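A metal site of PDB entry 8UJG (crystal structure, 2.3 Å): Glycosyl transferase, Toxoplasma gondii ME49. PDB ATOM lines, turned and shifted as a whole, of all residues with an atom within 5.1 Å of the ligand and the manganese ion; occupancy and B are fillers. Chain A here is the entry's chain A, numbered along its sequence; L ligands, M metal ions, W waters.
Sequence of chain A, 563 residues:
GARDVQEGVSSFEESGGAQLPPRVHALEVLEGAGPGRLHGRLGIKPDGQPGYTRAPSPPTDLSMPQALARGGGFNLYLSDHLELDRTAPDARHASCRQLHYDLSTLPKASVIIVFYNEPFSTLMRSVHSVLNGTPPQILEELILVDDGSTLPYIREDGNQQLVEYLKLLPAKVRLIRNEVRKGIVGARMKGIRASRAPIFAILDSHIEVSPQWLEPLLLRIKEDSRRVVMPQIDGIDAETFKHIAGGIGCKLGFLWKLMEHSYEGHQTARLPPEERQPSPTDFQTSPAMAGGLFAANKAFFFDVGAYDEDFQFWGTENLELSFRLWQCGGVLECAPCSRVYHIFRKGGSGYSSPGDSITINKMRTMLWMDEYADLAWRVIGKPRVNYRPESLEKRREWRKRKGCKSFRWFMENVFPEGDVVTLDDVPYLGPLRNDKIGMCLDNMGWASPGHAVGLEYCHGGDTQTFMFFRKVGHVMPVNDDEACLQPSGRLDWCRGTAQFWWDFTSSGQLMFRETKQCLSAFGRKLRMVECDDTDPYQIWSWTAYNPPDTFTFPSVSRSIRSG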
ATOM      1  N   VAL A 114      22.110  -3.982  14.534  1.00  0.00           N
ATOM      2  CA  VAL A 114      22.871  -2.861  14.013  1.00  0.00           C
ATOM      3  C   VAL A 114      22.689  -2.814  12.505  1.00  0.00           C
ATOM      4  O   VAL A 114      22.476  -3.853  11.855  1.00  0.00           O
ATOM      5  CB  VAL A 114      24.361  -2.956  14.401  1.00  0.00           C
ATOM      6  CG1 VAL A 114      24.501  -3.276  15.884  1.00  0.00           C
ATOM      7  CG2 VAL A 114      25.070  -4.002  13.561  1.00  0.00           C
ATOM      8  N   PHE A 115      22.761  -1.618  11.934  1.00  0.00           N
ATOM      9  CA  PHE A 115      22.519  -1.459  10.513  1.00  0.00           C
ATOM     10  C   PHE A 115      23.203  -0.193  10.019  1.00  0.00           C
ATOM     11  O   PHE A 115      23.234   0.820  10.722  1.00  0.00           O
ATOM     12  CB  PHE A 115      21.017  -1.380  10.219  1.00  0.00           C
ATOM     13  CG  PHE A 115      20.322  -0.240  10.898  1.00  0.00           C
ATOM     14  CD1 PHE A 115      19.865  -0.369  12.208  1.00  0.00           C
ATOM     15  CD2 PHE A 115      20.113   0.955  10.242  1.00  0.00           C
ATOM     16  CE1 PHE A 115      19.226   0.680  12.831  1.00  0.00           C
ATOM     17  CE2 PHE A 115      19.468   2.012  10.869  1.00  0.00           C
ATOM     18  CZ  PHE A 115      19.020   1.871  12.162  1.00  0.00           C
ATOM     19  N   TYR A 116      23.743  -0.255   8.804  1.00  0.00           N
ATOM     20  CA  TYR A 116      24.253   0.909   8.081  1.00  0.00           C
ATOM     21  C   TYR A 116      23.544   0.957   6.738  1.00  0.00           C
ATOM     22  O   TYR A 116      23.829   0.151   5.847  1.00  0.00           O
ATOM     23  CB  TYR A 116      25.772   0.855   7.914  1.00  0.00           C
ATOM     24  CG  TYR A 116      26.312   1.962   7.033  1.00  0.00           C
ATOM     25  CD1 TYR A 116      26.324   3.276   7.466  1.00  0.00           C
ATOM     26  CD2 TYR A 116      26.811   1.681   5.770  1.00  0.00           C
ATOM     27  CE1 TYR A 116      26.810   4.289   6.665  1.00  0.00           C
ATOM     28  CE2 TYR A 116      27.302   2.690   4.956  1.00  0.00           C
ATOM     29  CZ  TYR A 116      27.297   3.989   5.419  1.00  0.00           C
ATOM     30  OH  TYR A 116      27.791   5.008   4.619  1.00  0.00           O
ATOM     31  N   GLU A 118      20.519   0.197   5.919  1.00  0.00           N
ATOM     32  CA  GLU A 118      19.602  -0.893   5.618  1.00  0.00           C
ATOM     33  C   GLU A 118      18.261  -0.314   5.180  1.00  0.00           C
ATOM     34  O   GLU A 118      17.707   0.545   5.876  1.00  0.00           O
ATOM     35  CB  GLU A 118      19.413  -1.798   6.836  1.00  0.00           C
ATOM     36  CG  GLU A 118      18.586  -3.058   6.550  1.00  0.00           C
ATOM     37  CD  GLU A 118      19.347  -4.079   5.734  1.00  0.00           C
ATOM     38  OE1 GLU A 118      20.512  -4.367   6.088  1.00  0.00           O
ATOM     39  OE2 GLU A 118      18.794  -4.580   4.734  1.00  0.00           O
ATOM     40  N   ASP A 147      24.417   2.845  12.668  1.00  0.00           N
ATOM     41  CA  ASP A 147      25.863   3.030  12.586  1.00  0.00           C
ATOM     42  C   ASP A 147      26.220   4.106  11.560  1.00  0.00           C
ATOM     43  O   ASP A 147      26.862   3.864  10.550  1.00  0.00           O
ATOM     44  CB  ASP A 147      26.537   1.708  12.252  1.00  0.00           C
ATOM     45  CG  ASP A 147      28.050   1.788  12.335  1.00  0.00           C
ATOM     46  OD1 ASP A 147      28.558   2.644  13.080  1.00  0.00           O
ATOM     47  OD2 ASP A 147      28.722   1.007  11.629  1.00  0.00           O
ATOM     48  N   ARG A 181      29.949   6.551  11.286  1.00  0.00           N
ATOM     49  CA  ARG A 181      29.997   5.116  11.066  1.00  0.00           C
ATOM     50  C   ARG A 181      31.239   4.526  11.723  1.00  0.00           C
ATOM     51  O   ARG A 181      32.365   4.931  11.413  1.00  0.00           O
ATOM     52  CB  ARG A 181      30.012   4.816   9.572  1.00  0.00           C
ATOM     53  CG  ARG A 181      30.203   3.349   9.229  1.00  0.00           C
ATOM     54  CD  ARG A 181      30.312   3.144   7.735  1.00  0.00           C
ATOM     55  NE  ARG A 181      30.573   1.751   7.399  1.00  0.00           N
ATOM     56  CZ  ARG A 181      30.920   1.329   6.193  1.00  0.00           C
ATOM     57  NH1 ARG A 181      31.105   2.173   5.190  1.00  0.00           N
ATOM     58  NH2 ARG A 181      31.107   0.026   5.992  1.00  0.00           N
ATOM     59  N   GLY A 183      31.543   0.880  12.140  1.00  0.00           N
ATOM     60  CA  GLY A 183      31.751  -0.461  11.626  1.00  0.00           C
ATOM     61  C   GLY A 183      30.986  -1.492  12.434  1.00  0.00           C
ATOM     62  O   GLY A 183      30.287  -1.178  13.405  1.00  0.00           O
ATOM     63  N   ILE A 184      31.138  -2.748  12.017  1.00  0.00           N
ATOM     64  CA  ILE A 184      30.406  -3.837  12.644  1.00  0.00           C
ATOM     65  C   ILE A 184      30.744  -3.932  14.129  1.00  0.00           C
ATOM     66  O   ILE A 184      29.860  -3.988  14.984  1.00  0.00           O
ATOM     67  CB  ILE A 184      30.691  -5.169  11.914  1.00  0.00           C
ATOM     68  CG1 ILE A 184      29.754  -5.306  10.710  1.00  0.00           C
ATOM     69  CG2 ILE A 184      30.527  -6.359  12.863  1.00  0.00           C
ATOM     70  CD1 ILE A 184      30.038  -6.506   9.826  1.00  0.00           C
ATOM     71  N   ALA A 187      29.625  -0.778  16.072  1.00  0.00           N
ATOM     72  CA  ALA A 187      28.172  -0.703  16.160  1.00  0.00           C
ATOM     73  C   ALA A 187      27.627  -1.712  17.157  1.00  0.00           C
ATOM     74  O   ALA A 187      26.755  -1.386  17.967  1.00  0.00           O
ATOM     75  CB  ALA A 187      27.548  -0.935  14.778  1.00  0.00           C
ATOM     76  N   ARG A 188      28.139  -2.947  17.125  1.00  0.00           N
ATOM     77  CA  ARG A 188      27.642  -3.962  18.046  1.00  0.00           C
ATOM     78  C   ARG A 188      28.005  -3.640  19.486  1.00  0.00           C
ATOM     79  O   ARG A 188      27.193  -3.849  20.399  1.00  0.00           O
ATOM     80  CB  ARG A 188      28.195  -5.331  17.660  1.00  0.00           C
ATOM     81  CG  ARG A 188      27.608  -5.862  16.360  1.00  0.00           C
ATOM     82  CD  ARG A 188      28.189  -7.222  15.994  1.00  0.00           C
ATOM     83  NE  ARG A 188      27.687  -7.664  14.694  1.00  0.00           N
ATOM     84  CZ  ARG A 188      28.249  -8.617  13.959  1.00  0.00           C
ATOM     85  NH1 ARG A 188      29.332  -9.258  14.361  1.00  0.00           N
ATOM     86  NH2 ARG A 188      27.706  -8.930  12.793  1.00  0.00           N
ATOM     87  N   ASP A 204      21.188  -9.823  12.289  1.00  0.00           N
ATOM     88  CA  ASP A 204      21.381  -8.935  11.162  1.00  0.00           C
ATOM     89  C   ASP A 204      20.106  -8.125  10.914  1.00  0.00           C
ATOM     90  O   ASP A 204      19.027  -8.451  11.422  1.00  0.00           O
ATOM     91  CB  ASP A 204      21.763  -9.705   9.898  1.00  0.00           C
ATOM     92  CG  ASP A 204      23.246 -10.044   9.842  1.00  0.00           C
ATOM     93  OD1 ASP A 204      23.899  -9.988  10.909  1.00  0.00           O
ATOM     94  OD2 ASP A 204      23.740 -10.359   8.740  1.00  0.00           O
ATOM     95  N   SER A 205      20.231  -7.079  10.110  1.00  0.00           N
ATOM     96  CA  SER A 205      19.129  -6.178   9.826  1.00  0.00           C
ATOM     97  C   SER A 205      18.306  -6.606   8.617  1.00  0.00           C
ATOM     98  O   SER A 205      17.541  -5.806   8.073  1.00  0.00           O
ATOM     99  CB  SER A 205      19.664  -4.752   9.617  1.00  0.00           C
ATOM    100  OG  SER A 205      20.669  -4.728   8.630  1.00  0.00           O
ATOM    101  N   HIS A 206      18.459  -7.859   8.170  1.00  0.00           N
ATOM    102  CA  HIS A 206      17.750  -8.411   7.024  1.00  0.00           C
ATOM    103  C   HIS A 206      17.487  -9.891   7.307  1.00  0.00           C
ATOM    104  O   HIS A 206      18.027 -10.792   6.673  1.00  0.00           O
ATOM    105  CB  HIS A 206      18.551  -8.202   5.731  1.00  0.00           C
ATOM    106  CG  HIS A 206      20.034  -8.311   5.929  1.00  0.00           C
ATOM    107  ND1 HIS A 206      20.854  -7.203   5.981  1.00  0.00           N
ATOM    108  CD2 HIS A 206      20.841  -9.382   6.075  1.00  0.00           C
ATOM    109  CE1 HIS A 206      22.100  -7.585   6.165  1.00  0.00           C
ATOM    110  NE2 HIS A 206      22.129  -8.909   6.222  1.00  0.00           N
ATOM    111  N   PHE A 313      35.651  -1.311  10.263  1.00  0.00           N
ATOM    112  CA  PHE A 313      34.556  -1.486   9.321  1.00  0.00           C
ATOM    113  C   PHE A 313      34.075  -2.940   9.303  1.00  0.00           C
ATOM    114  O   PHE A 313      33.454  -3.384  10.265  1.00  0.00           O
ATOM    115  CB  PHE A 313      35.000  -1.004   7.935  1.00  0.00           C
ATOM    116  CG  PHE A 313      35.208   0.492   7.853  1.00  0.00           C
ATOM    117  CD1 PHE A 313      34.120   1.350   7.723  1.00  0.00           C
ATOM    118  CD2 PHE A 313      36.475   1.043   7.924  1.00  0.00           C
ATOM    119  CE1 PHE A 313      34.300   2.722   7.661  1.00  0.00           C
ATOM    120  CE2 PHE A 313      36.660   2.411   7.849  1.00  0.00           C
ATOM    121  CZ  PHE A 313      35.570   3.253   7.724  1.00  0.00           C
ATOM    122  N   TRP A 314      34.358  -3.681   8.231  1.00  0.00           N
ATOM    123  CA  TRP A 314      33.749  -4.985   8.000  1.00  0.00           C
ATOM    124  C   TRP A 314      34.802  -6.082   7.921  1.00  0.00           C
ATOM    125  O   TRP A 314      35.875  -5.879   7.331  1.00  0.00           O
ATOM    126  CB  TRP A 314      32.910  -4.966   6.710  1.00  0.00           C
ATOM    127  CG  TRP A 314      32.194  -6.245   6.409  1.00  0.00           C
ATOM    128  CD1 TRP A 314      30.882  -6.534   6.700  1.00  0.00           C
ATOM    129  CD2 TRP A 314      32.719  -7.409   5.771  1.00  0.00           C
ATOM    130  NE1 TRP A 314      30.577  -7.811   6.276  1.00  0.00           N
ATOM    131  CE2 TRP A 314      31.690  -8.367   5.704  1.00  0.00           C
ATOM    132  CE3 TRP A 314      33.975  -7.737   5.245  1.00  0.00           C
ATOM    133  CZ2 TRP A 314      31.869  -9.622   5.143  1.00  0.00           C
ATOM    134  CZ3 TRP A 314      34.154  -8.992   4.683  1.00  0.00           C
ATOM    135  CH2 TRP A 314      33.103  -9.920   4.632  1.00  0.00           C
ATOM    136  N   HIS A 342      18.054 -15.511   6.698  1.00  0.00           N
ATOM    137  CA  HIS A 342      18.990 -14.436   6.435  1.00  0.00           C
ATOM    138  C   HIS A 342      19.098 -14.210   4.938  1.00  0.00           C
ATOM    139  O   HIS A 342      19.214 -15.163   4.170  1.00  0.00           O
ATOM    140  CB  HIS A 342      20.377 -14.747   7.015  1.00  0.00           C
ATOM    141  CG  HIS A 342      21.420 -13.731   6.678  1.00  0.00           C
ATOM    142  ND1 HIS A 342      22.203 -13.806   5.547  1.00  0.00           N
ATOM    143  CD2 HIS A 342      21.826 -12.621   7.334  1.00  0.00           C
ATOM    144  CE1 HIS A 342      23.039 -12.781   5.521  1.00  0.00           C
ATOM    145  NE2 HIS A 342      22.829 -12.040   6.591  1.00  0.00           N
ATOM    146  N   ILE A 343      19.047 -12.945   4.524  1.00  0.00           N
ATOM    147  CA  ILE A 343      19.223 -12.585   3.124  1.00  0.00           C
ATOM    148  C   ILE A 343      20.720 -12.550   2.832  1.00  0.00           C
ATOM    149  O   ILE A 343      21.440 -11.684   3.339  1.00  0.00           O
ATOM    150  CB  ILE A 343      18.557 -11.245   2.788  1.00  0.00           C
ATOM    151  CG1 ILE A 343      17.073 -11.255   3.153  1.00  0.00           C
ATOM    152  CG2 ILE A 343      18.724 -10.930   1.306  1.00  0.00           C
ATOM    153  CD1 ILE A 343      16.394  -9.905   2.987  1.00  0.00           C
ATOM    154  N   ARG A 345      23.488 -11.659   0.173  1.00  0.00           N
ATOM    155  CA  ARG A 345      23.448 -10.750  -0.962  1.00  0.00           C
ATOM    156  C   ARG A 345      23.934 -11.459  -2.219  1.00  0.00           C
ATOM    157  O   ARG A 345      24.746 -12.380  -2.176  1.00  0.00           O
ATOM    158  CB  ARG A 345      24.324  -9.523  -0.697  1.00  0.00           C
ATOM    159  CG  ARG A 345      24.014  -8.831   0.610  1.00  0.00           C
ATOM    160  CD  ARG A 345      24.861  -7.590   0.831  1.00  0.00           C
ATOM    161  NE  ARG A 345      24.861  -7.191   2.231  1.00  0.00           N
ATOM    162  CZ  ARG A 345      24.093  -6.238   2.728  1.00  0.00           C
ATOM    163  NH1 ARG A 345      23.110  -5.699   2.018  1.00  0.00           N
ATOM    164  NH2 ARG A 345      24.263  -5.854   3.985  1.00  0.00           N
ATOM    165  N   TYR A 351      26.958  -1.548   1.008  1.00  0.00           N
ATOM    166  CA  TYR A 351      27.862  -0.496   1.438  1.00  0.00           C
ATOM    167  C   TYR A 351      29.271  -0.865   1.001  1.00  0.00           C
ATOM    168  O   TYR A 351      29.564  -2.027   0.729  1.00  0.00           O
ATOM    169  CB  TYR A 351      27.818  -0.300   2.961  1.00  0.00           C
ATOM    170  CG  TYR A 351      27.965  -1.598   3.728  1.00  0.00           C
ATOM    171  CD1 TYR A 351      29.217  -2.143   3.976  1.00  0.00           C
ATOM    172  CD2 TYR A 351      26.848  -2.272   4.181  1.00  0.00           C
ATOM    173  CE1 TYR A 351      29.355  -3.329   4.669  1.00  0.00           C
ATOM    174  CE2 TYR A 351      26.978  -3.463   4.872  1.00  0.00           C
ATOM    175  CZ  TYR A 351      28.226  -3.984   5.120  1.00  0.00           C
ATOM    176  OH  TYR A 351      28.349  -5.164   5.807  1.00  0.00           O
HETATM  177  N1  LIG L   1      26.815  -3.100   9.444  1.00  0.00           N
HETATM  178  C1  LIG L   1      26.941  -1.949  10.197  1.00  0.00           C
HETATM  179  N2  LIG L   1      28.035  -1.176   9.907  1.00  0.00           N
HETATM  180  C2  LIG L   1      28.999  -1.436   8.945  1.00  0.00           C
HETATM  181  C3  LIG L   1      28.794  -2.653   8.212  1.00  0.00           C
HETATM  182  C4  LIG L   1      27.730  -3.431   8.473  1.00  0.00           C
HETATM  183  O1  LIG L   1      26.141  -1.630  11.068  1.00  0.00           O
HETATM  184  O2  LIG L   1      29.933  -0.645   8.786  1.00  0.00           O
HETATM  185  C5  LIG L   1      25.659  -3.976   9.715  1.00  0.00           C
HETATM  186  C6  LIG L   1      24.905  -4.410   8.460  1.00  0.00           C
HETATM  187  O3  LIG L   1      23.924  -3.461   8.098  1.00  0.00           O
HETATM  188  C7  LIG L   1      24.281  -5.724   8.924  1.00  0.00           C
HETATM  189  C8  LIG L   1      25.336  -6.298   9.880  1.00  0.00           C
HETATM  190  O4  LIG L   1      26.127  -5.169  10.316  1.00  0.00           O
HETATM  191  O5  LIG L   1      23.047  -5.522   9.593  1.00  0.00           O
HETATM  192  C9  LIG L   1      26.234  -7.356   9.276  1.00  0.00           C
HETATM  193  O6  LIG L   1      26.670  -6.945   7.962  1.00  0.00           O
HETATM  194  P1  LIG L   1      26.354  -7.826   6.684  1.00  0.00           P
HETATM  195  O7  LIG L   1      24.937  -8.234   6.770  1.00  0.00           O
HETATM  196  O8  LIG L   1      26.798  -7.110   5.413  1.00  0.00           O
HETATM  197  O9  LIG L   1      27.305  -9.093   6.838  1.00  0.00           O
HETATM  198  P2  LIG L   1      27.238 -10.334   5.854  1.00  0.00           P
HETATM  199  O10 LIG L   1      28.596 -11.012   6.065  1.00  0.00           O
HETATM  200  O11 LIG L   1      26.122 -11.191   6.452  1.00  0.00           O
HETATM  201  O12 LIG L   1      26.989  -9.915   4.440  1.00  0.00           O
HETATM  202 MN    MN M   1      23.980 -10.123   6.583  1.00  0.00          MN
HETATM  203  O   HOH W   1      23.000  -3.284   5.274  1.00  0.00           O
HETATM  204  O   HOH W   2      24.065 -10.278   4.394  1.00  0.00           O
HETATM  205  O   HOH W   3      22.995  -6.514  12.899  1.00  0.00           O
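A ring nitrogen (ND1) of His 206 is in hydrogen-bond range of the side-chain carboxylate (OE1) of Glu 118.
The backbone carbonyl oxygen of His 206 is in hydrogen-bond range of the backbone NH of Ile 343 (3.2 Å).
The side-chain hydroxyl of Tyr 351 lies close to the indole nitrogen of Trp 314.
OG of Ser 205 is in hydrogen-bond range of OE1 of Glu 118.
N of Gly 183 lies within hydrogen-bond range of OD2 of Asp 147 (2.9 Å).
N of Asp 147 sits at hydrogen-bond distance from O of Phe 115 (3.0 Å).
O of Phe 313 is in hydrogen-bond range of N of Ile 184 (3.0 Å).
Of the 19 residues printed, 3 come within 4 Å of the manganese ion.
The nearest printed residue that does not touch the manganese ion is Ile 343 (4.4 Å).
CA of Gly 183 touches O2 of the ligand (3.4 Å).
Ile 184 touches the ligand.
NE1 of Trp 314 touches O9 of the ligand (3.6 Å).
Hydrophobic or aromatic side chains within 4 Å of the ligand: Val 114, Tyr 116, Ile 184, His 206, Trp 314, His 342 and Tyr 351.
Within 4 Å of the ligand: Val 114, Phe 115, Tyr 116, Asp 147, Arg 181, Gly 183, Ile 184, Asp 204, Ser 205, His 206, Trp 314, His 342, Arg 345 and Tyr 351.
Water W2 bridges an oxygen (O12) of the ligand and the backbone carbonyl oxygen (O) of Ile 343.
Water W1 lies within hydrogen-bond range of the side-chain carboxylate of Glu 118, an oxygen (O3) of the ligand and the guanidinium group of Arg 345.
Water W3 lies within hydrogen-bond range of the backbone carbonyl oxygen (O) of Val 114 (2.9 Å) and an oxygen (O5) of the ligand (3.5 Å).
O8 of the ligand lies within hydrogen-bond range of OH of Tyr 351, at 2.5 Å.
O5 of the ligand is in hydrogen-bond range of N of Ser 205 (3.3 Å).
An oxygen (O5) of the ligand lies within hydrogen-bond range of the side-chain hydroxyl of Ser 205, at 2.7 Å.
The guanidinium group (NE) of Arg 181 lies within hydrogen-bond range of an oxygen (O2) of the ligand, at 2.8 Å.
OD2 of Asp 147 is in hydrogen-bond range of N2 of the ligand (2.9 Å).
The backbone carbonyl oxygen (O) of Val 114 is in hydrogen-bond range of an oxygen (O5) of the ligand, at 2.9 Å.
NH2 of Arg 345 lies within salt-bridge range of O8 of the ligand, at 3.2 Å.
N of Tyr 116 lies within hydrogen-bond range of O3 of the ligand (3.3 Å).
An oxygen (O1) of the ligand lies close to the backbone NH (N) of Phe 115, 3.5 Å away.
O7 of the ligand is bound to the manganese ion.
OD2 of Asp 204 is bound to the manganese ion, at 2.2 Å.
Water W2 is bound to the manganese ion, 2.2 Å away.
A ring nitrogen (NE2) of His 342 binds the manganese ion, 2.2 Å away.
A ring nitrogen (NE2) of His 206 binds the manganese ion, at 2.2 Å.
An oxygen (O11) of the ligand binds the manganese ion.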
